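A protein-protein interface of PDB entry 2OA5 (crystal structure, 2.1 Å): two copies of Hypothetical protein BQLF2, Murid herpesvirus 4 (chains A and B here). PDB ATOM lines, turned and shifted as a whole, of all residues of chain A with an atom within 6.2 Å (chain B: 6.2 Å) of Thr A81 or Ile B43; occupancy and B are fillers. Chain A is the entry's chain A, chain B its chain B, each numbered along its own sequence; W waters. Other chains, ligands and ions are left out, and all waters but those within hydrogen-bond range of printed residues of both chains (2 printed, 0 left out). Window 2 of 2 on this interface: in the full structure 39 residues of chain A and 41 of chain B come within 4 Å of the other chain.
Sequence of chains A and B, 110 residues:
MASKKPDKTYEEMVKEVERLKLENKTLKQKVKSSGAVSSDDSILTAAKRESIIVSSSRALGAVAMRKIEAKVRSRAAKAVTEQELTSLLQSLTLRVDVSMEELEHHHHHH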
ATOM      1  N   LYS A  78     -24.453 -22.965 -22.838  1.00  0.00           N
ATOM      2  CA  LYS A  78     -24.045 -24.046 -21.936  1.00  0.00           C
ATOM      3  C   LYS A  78     -22.855 -24.890 -22.415  1.00  0.00           C
ATOM      4  O   LYS A  78     -22.245 -25.606 -21.617  1.00  0.00           O
ATOM      5  CB  LYS A  78     -25.237 -24.971 -21.654  1.00  0.00           C
ATOM      6  CG  LYS A  78     -25.647 -25.833 -22.839  1.00  0.00           C
ATOM      7  CD  LYS A  78     -26.948 -26.575 -22.579  1.00  0.00           C
ATOM      8  CE  LYS A  78     -27.309 -27.481 -23.752  1.00  0.00           C
ATOM      9  NZ  LYS A  78     -28.710 -27.988 -23.646  1.00  0.00           N
ATOM     10  N   ALA A  79     -22.522 -24.820 -23.702  1.00  0.00           N
ATOM     11  CA  ALA A  79     -21.405 -25.604 -24.231  1.00  0.00           C
ATOM     12  C   ALA A  79     -20.052 -25.066 -23.765  1.00  0.00           C
ATOM     13  O   ALA A  79     -19.814 -23.859 -23.805  1.00  0.00           O
ATOM     14  CB  ALA A  79     -21.462 -25.624 -25.753  1.00  0.00           C
ATOM     15  N   VAL A  80     -19.171 -25.963 -23.315  1.00  0.00           N
ATOM     16  CA  VAL A  80     -17.833 -25.590 -22.849  1.00  0.00           C
ATOM     17  C   VAL A  80     -16.750 -26.171 -23.765  1.00  0.00           C
ATOM     18  O   VAL A  80     -15.718 -25.538 -23.986  1.00  0.00           O
ATOM     19  CB  VAL A  80     -17.590 -26.061 -21.384  1.00  0.00           C
ATOM     20  CG1 VAL A  80     -16.108 -26.156 -21.083  1.00  0.00           C
ATOM     21  CG2 VAL A  80     -18.208 -25.072 -20.424  1.00  0.00           C
ATOM     22  N   THR A  81     -16.987 -27.368 -24.301  1.00  0.00           N
ATOM     23  CA  THR A  81     -16.018 -28.000 -25.202  1.00  0.00           C
ATOM     24  C   THR A  81     -16.436 -27.882 -26.672  1.00  0.00           C
ATOM     25  O   THR A  81     -17.588 -27.572 -26.984  1.00  0.00           O
ATOM     26  CB  THR A  81     -15.811 -29.516 -24.880  1.00  0.00           C
ATOM     27  OG1 THR A  81     -17.019 -30.241 -25.142  1.00  0.00           O
ATOM     28  CG2 THR A  81     -15.436 -29.716 -23.427  1.00  0.00           C
ATOM     29  N   GLU A  82     -15.485 -28.146 -27.566  1.00  0.00           N
ATOM     30  CA  GLU A  82     -15.704 -28.077 -29.012  1.00  0.00           C
ATOM     31  C   GLU A  82     -16.728 -29.110 -29.468  1.00  0.00           C
ATOM     32  O   GLU A  82     -17.697 -28.791 -30.169  1.00  0.00           O
ATOM     33  CB  GLU A  82     -14.376 -28.307 -29.740  1.00  0.00           C
ATOM     34  CG  GLU A  82     -13.264 -27.368 -29.285  1.00  0.00           C
ATOM     35  CD  GLU A  82     -11.939 -27.629 -29.970  1.00  0.00           C
ATOM     36  OE1 GLU A  82     -11.818 -28.662 -30.661  1.00  0.00           O
ATOM     37  OE2 GLU A  82     -11.011 -26.806 -29.811  1.00  0.00           O
ATOM     38  N   GLN A  83     -16.495 -30.352 -29.067  1.00  0.00           N
ATOM     39  CA  GLN A  83     -17.383 -31.446 -29.410  1.00  0.00           C
ATOM     40  C   GLN A  83     -18.767 -31.107 -28.842  1.00  0.00           C
ATOM     41  O   GLN A  83     -19.798 -31.430 -29.437  1.00  0.00           O
ATOM     42  CB  GLN A  83     -16.869 -32.766 -28.800  1.00  0.00           C
ATOM     43  CG  GLN A  83     -15.357 -33.058 -28.951  1.00  0.00           C
ATOM     44  CD  GLN A  83     -14.902 -33.250 -30.387  1.00  0.00           C
ATOM     45  OE1 GLN A  83     -15.634 -33.790 -31.215  1.00  0.00           O
ATOM     46  NE2 GLN A  83     -13.673 -32.829 -30.683  1.00  0.00           N
ATOM     47  N   GLU A  84     -18.775 -30.449 -27.684  1.00  0.00           N
ATOM     48  CA  GLU A  84     -20.019 -30.040 -27.026  1.00  0.00           C
ATOM     49  C   GLU A  84     -20.769 -28.987 -27.835  1.00  0.00           C
ATOM     50  O   GLU A  84     -21.980 -29.096 -28.037  1.00  0.00           O
ATOM     51  CB  GLU A  84     -19.731 -29.492 -25.624  1.00  0.00           C
ATOM     52  CG  GLU A  84     -19.890 -30.518 -24.509  1.00  0.00           C
ATOM     53  CD  GLU A  84     -19.420 -30.000 -23.164  1.00  0.00           C
ATOM     54  OE1 GLU A  84     -19.043 -28.811 -23.088  1.00  0.00           O
ATOM     55  OE2 GLU A  84     -19.426 -30.779 -22.185  1.00  0.00           O
ATOM     56  N   LEU A  85     -20.044 -27.966 -28.286  1.00  0.00           N
ATOM     57  CA  LEU A  85     -20.635 -26.886 -29.073  1.00  0.00           C
ATOM     58  C   LEU A  85     -21.086 -27.434 -30.426  1.00  0.00           C
ATOM     59  O   LEU A  85     -22.229 -27.225 -30.852  1.00  0.00           O
ATOM     60  CB  LEU A  85     -19.620 -25.757 -29.273  1.00  0.00           C
ATOM     61  CG  LEU A  85     -20.140 -24.548 -30.060  1.00  0.00           C
ATOM     62  CD1 LEU A  85     -21.396 -24.023 -29.394  1.00  0.00           C
ATOM     63  CD2 LEU A  85     -19.089 -23.456 -30.110  1.00  0.00           C
ATOM     64  N   THR A  86     -20.178 -28.154 -31.082  1.00  0.00           N
ATOM     65  CA  THR A  86     -20.439 -28.765 -32.382  1.00  0.00           C
ATOM     66  C   THR A  86     -21.709 -29.611 -32.379  1.00  0.00           C
ATOM     67  O   THR A  86     -22.546 -29.500 -33.274  1.00  0.00           O
ATOM     68  CB  THR A  86     -19.238 -29.642 -32.828  1.00  0.00           C
ATOM     69  OG1 THR A  86     -18.246 -28.816 -33.444  1.00  0.00           O
ATOM     70  CG2 THR A  86     -19.672 -30.704 -33.820  1.00  0.00           C
ATOM     71  N   LYS B  28     -12.462 -23.719 -15.239  1.00  0.00           N
ATOM     72  CA  LYS B  28     -11.891 -24.364 -16.416  1.00  0.00           C
ATOM     73  C   LYS B  28     -10.558 -24.956 -15.995  1.00  0.00           C
ATOM     74  O   LYS B  28     -10.177 -26.038 -16.430  1.00  0.00           O
ATOM     75  CB  LYS B  28     -11.680 -23.353 -17.544  1.00  0.00           C
ATOM     76  CG  LYS B  28     -12.925 -23.135 -18.388  1.00  0.00           C
ATOM     77  CD  LYS B  28     -12.785 -21.924 -19.285  1.00  0.00           C
ATOM     78  CE  LYS B  28     -14.066 -21.686 -20.058  1.00  0.00           C
ATOM     79  NZ  LYS B  28     -14.021 -20.419 -20.829  1.00  0.00           N
ATOM     80  N   VAL B  31     -11.195 -28.157 -14.274  1.00  0.00           N
ATOM     81  CA  VAL B  31     -11.694 -29.123 -15.248  1.00  0.00           C
ATOM     82  C   VAL B  31     -10.525 -29.698 -16.050  1.00  0.00           C
ATOM     83  O   VAL B  31     -10.535 -30.869 -16.420  1.00  0.00           O
ATOM     84  CB  VAL B  31     -12.730 -28.477 -16.220  1.00  0.00           C
ATOM     85  CG1 VAL B  31     -12.752 -29.226 -17.546  1.00  0.00           C
ATOM     86  CG2 VAL B  31     -14.121 -28.517 -15.604  1.00  0.00           C
ATOM     87  N   LYS B  32      -9.523 -28.865 -16.314  1.00  0.00           N
ATOM     88  CA  LYS B  32      -8.344 -29.289 -17.061  1.00  0.00           C
ATOM     89  C   LYS B  32      -7.410 -30.078 -16.159  1.00  0.00           C
ATOM     90  O   LYS B  32      -6.933 -31.148 -16.541  1.00  0.00           O
ATOM     91  CB  LYS B  32      -7.592 -28.082 -17.604  1.00  0.00           C
ATOM     92  CG  LYS B  32      -8.201 -27.469 -18.830  1.00  0.00           C
ATOM     93  CD  LYS B  32      -8.134 -25.974 -18.710  1.00  0.00           C
ATOM     94  CE  LYS B  32      -7.823 -25.328 -20.030  1.00  0.00           C
ATOM     95  NZ  LYS B  32      -7.780 -23.866 -19.837  1.00  0.00           N
ATOM     96  N   ALA B  36     -11.037 -34.250 -16.676  1.00  0.00           N
ATOM     97  CA  ALA B  36     -12.346 -34.439 -17.289  1.00  0.00           C
ATOM     98  C   ALA B  36     -12.434 -33.722 -18.632  1.00  0.00           C
ATOM     99  O   ALA B  36     -13.566 -33.198 -18.943  1.00  0.00           O
ATOM    100  CB  ALA B  36     -13.444 -33.955 -16.355  1.00  0.00           C
ATOM    101  N   VAL B  37     -11.434 -33.787 -19.405  1.00  0.00           N
ATOM    102  CA  VAL B  37     -11.484 -33.267 -20.746  1.00  0.00           C
ATOM    103  C   VAL B  37     -10.796 -34.313 -21.587  1.00  0.00           C
ATOM    104  O   VAL B  37      -9.569 -34.499 -21.583  1.00  0.00           O
ATOM    105  CB  VAL B  37     -10.856 -31.856 -20.930  1.00  0.00           C
ATOM    106  CG1 VAL B  37      -9.377 -31.932 -21.293  1.00  0.00           C
ATOM    107  CG2 VAL B  37     -11.637 -31.121 -22.026  1.00  0.00           C
ATOM    108  N   ASP B  41     -11.133 -34.451 -26.993  1.00  0.00           N
ATOM    109  CA  ASP B  41     -11.803 -33.160 -26.942  1.00  0.00           C
ATOM    110  C   ASP B  41     -10.915 -32.007 -26.497  1.00  0.00           C
ATOM    111  O   ASP B  41      -9.697 -32.137 -26.342  1.00  0.00           O
ATOM    112  CB  ASP B  41     -12.999 -33.242 -25.998  1.00  0.00           C
ATOM    113  CG  ASP B  41     -14.049 -32.189 -26.282  1.00  0.00           C
ATOM    114  OD1 ASP B  41     -13.750 -31.209 -27.000  1.00  0.00           O
ATOM    115  OD2 ASP B  41     -15.183 -32.344 -25.783  1.00  0.00           O
ATOM    116  N   SER B  42     -11.562 -30.870 -26.269  1.00  0.00           N
ATOM    117  CA  SER B  42     -10.873 -29.677 -25.842  1.00  0.00           C
ATOM    118  C   SER B  42     -11.851 -28.646 -25.302  1.00  0.00           C
ATOM    119  O   SER B  42     -13.028 -28.621 -25.667  1.00  0.00           O
ATOM    120  CB  SER B  42     -10.102 -29.072 -27.013  1.00  0.00           C
ATOM    121  OG  SER B  42      -9.352 -27.944 -26.596  1.00  0.00           O
ATOM    122  N   ILE B  43     -11.348 -27.806 -24.408  1.00  0.00           N
ATOM    123  CA  ILE B  43     -12.143 -26.740 -23.840  1.00  0.00           C
ATOM    124  C   ILE B  43     -12.031 -25.612 -24.858  1.00  0.00           C
ATOM    125  O   ILE B  43     -10.954 -25.323 -25.386  1.00  0.00           O
ATOM    126  CB  ILE B  43     -11.607 -26.306 -22.442  1.00  0.00           C
ATOM    127  CG1 ILE B  43     -12.338 -27.064 -21.329  1.00  0.00           C
ATOM    128  CG2 ILE B  43     -11.887 -24.829 -22.202  1.00  0.00           C
ATOM    129  CD1 ILE B  43     -12.879 -28.413 -21.721  1.00  0.00           C
ATOM    130  N   LEU B  44     -13.174 -25.005 -25.141  1.00  0.00           N
ATOM    131  CA  LEU B  44     -13.293 -23.928 -26.106  1.00  0.00           C
ATOM    132  C   LEU B  44     -12.600 -22.636 -25.685  1.00  0.00           C
ATOM    133  O   LEU B  44     -12.766 -22.175 -24.552  1.00  0.00           O
ATOM    134  CB  LEU B  44     -14.791 -23.646 -26.325  1.00  0.00           C
ATOM    135  CG  LEU B  44     -15.501 -23.768 -27.675  1.00  0.00           C
ATOM    136  CD1 LEU B  44     -14.922 -24.884 -28.489  1.00  0.00           C
ATOM    137  CD2 LEU B  44     -16.987 -23.994 -27.426  1.00  0.00           C
ATOM    138  N   THR B  45     -11.799 -22.074 -26.588  1.00  0.00           N
ATOM    139  CA  THR B  45     -11.174 -20.778 -26.331  1.00  0.00           C
ATOM    140  C   THR B  45     -12.281 -19.804 -26.784  1.00  0.00           C
ATOM    141  O   THR B  45     -13.148 -20.180 -27.569  1.00  0.00           O
ATOM    142  CB  THR B  45      -9.908 -20.529 -27.195  1.00  0.00           C
ATOM    143  OG1 THR B  45     -10.236 -20.662 -28.580  1.00  0.00           O
ATOM    144  CG2 THR B  45      -8.782 -21.511 -26.824  1.00  0.00           C
HETATM  145  O   HOH W   1     -11.262 -24.685 -28.286  1.00  0.00           O
HETATM  146  O   HOH W   2     -14.845 -22.844 -22.533  1.00  0.00           O
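The backbone carbonyl oxygen of Val A80 is in hydrogen-bond range of the backbone NH of Leu B44 (2.8 Å). The side-chain carboxylate (OD2) of Asp B41 is in hydrogen-bond range of the side-chain hydroxyl (OG1) of Thr A81 (2.9 Å). O of Ser B42 is in hydrogen-bond range of N of Glu A82 (3.1 Å).
The backbone NH (N) of Val A80 lies within hydrogen-bond range of the side-chain carboxylate (OE1) of Glu A84, 2.9 Å away. The backbone NH (N) of Thr A81 sits at hydrogen-bond distance from the side-chain carboxylate (OE1) of Glu A84, at 2.8 Å. The backbone carbonyl oxygen of Glu A82 lies close to the side-chain hydroxyl of Thr A86.
Ile B43 touches Val A80 (CA to O, 3.8 Å). O of Ser B42 touches CB of Thr A81 (3.0 Å). Thr A81 touches Ile B43 (CG2 to CD1, 3.3 Å). Leu B44 touches Thr A81. Asp B41 touches Glu A82. Glu A82 touches Leu B44. Gln A83 touches Asp B41. Leu A85 touches Leu B44.
Thr A81 touches just these residues of chain B: Asp B41 (2.9 Å), Ser B42 (3.0 Å), Ile B43 (3.3 Å) and Leu B44 (3.7 Å). Ile B43 touches just these residues of chain A: Val A80 (3.8 Å) and Thr A81 (3.3 Å). Printed residues of chain B within 4 Å of Glu A82: Asp B41 (3.6 Å), Ser B42 (3.1 Å) and Leu B44 (3.1 Å). Printed residues of chain A within 4 Å of Leu B44: Val A80 (2.8 Å), Thr A81 (3.7 Å), Glu A82 (3.1 Å) and Leu A85 (3.5 Å). Of the printed residues of chain B, Val A80 touches Ile B43 and Leu B44. Printed residues of chain A within 4 Å of Asp B41: Thr A81, Glu A82 and Gln A83. Of the printed residues of chain B, Leu A85 touches Leu B44 (3.5 Å). The nearest printed residue of chain B that does not touch Val A80 is Ser B42 (4.4 Å).
Hydrophobic or aromatic side chains of chain B that line the printed part of chain A: Ile B43 and Leu B44. Hydrophobic or aromatic side chains of chain A within 4 Å of the printed part of chain B: Val A80 and Leu A85. Among the printed residues, no Asp or Glu carboxylate lies within 4 Å of a Lys or Arg side-chain nitrogen of the other chain.
No position is printed for both chains. Of the 11 pairs that touch across the chains among the printed residues, none has its exchanged pair printed and touching as well.
Water W1 lies within hydrogen-bond range of OE2 of Glu A82 (2.6 Å), O of Ile B43 (3.0 Å) and N of Thr B45 (3.2 Å). Water W2 lies within hydrogen-bond range of the backbone carbonyl oxygen (O) of Leu B44, the side-chain amino group (NZ) of Lys B28 and the backbone carbonyl oxygen (O) of Val A80.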
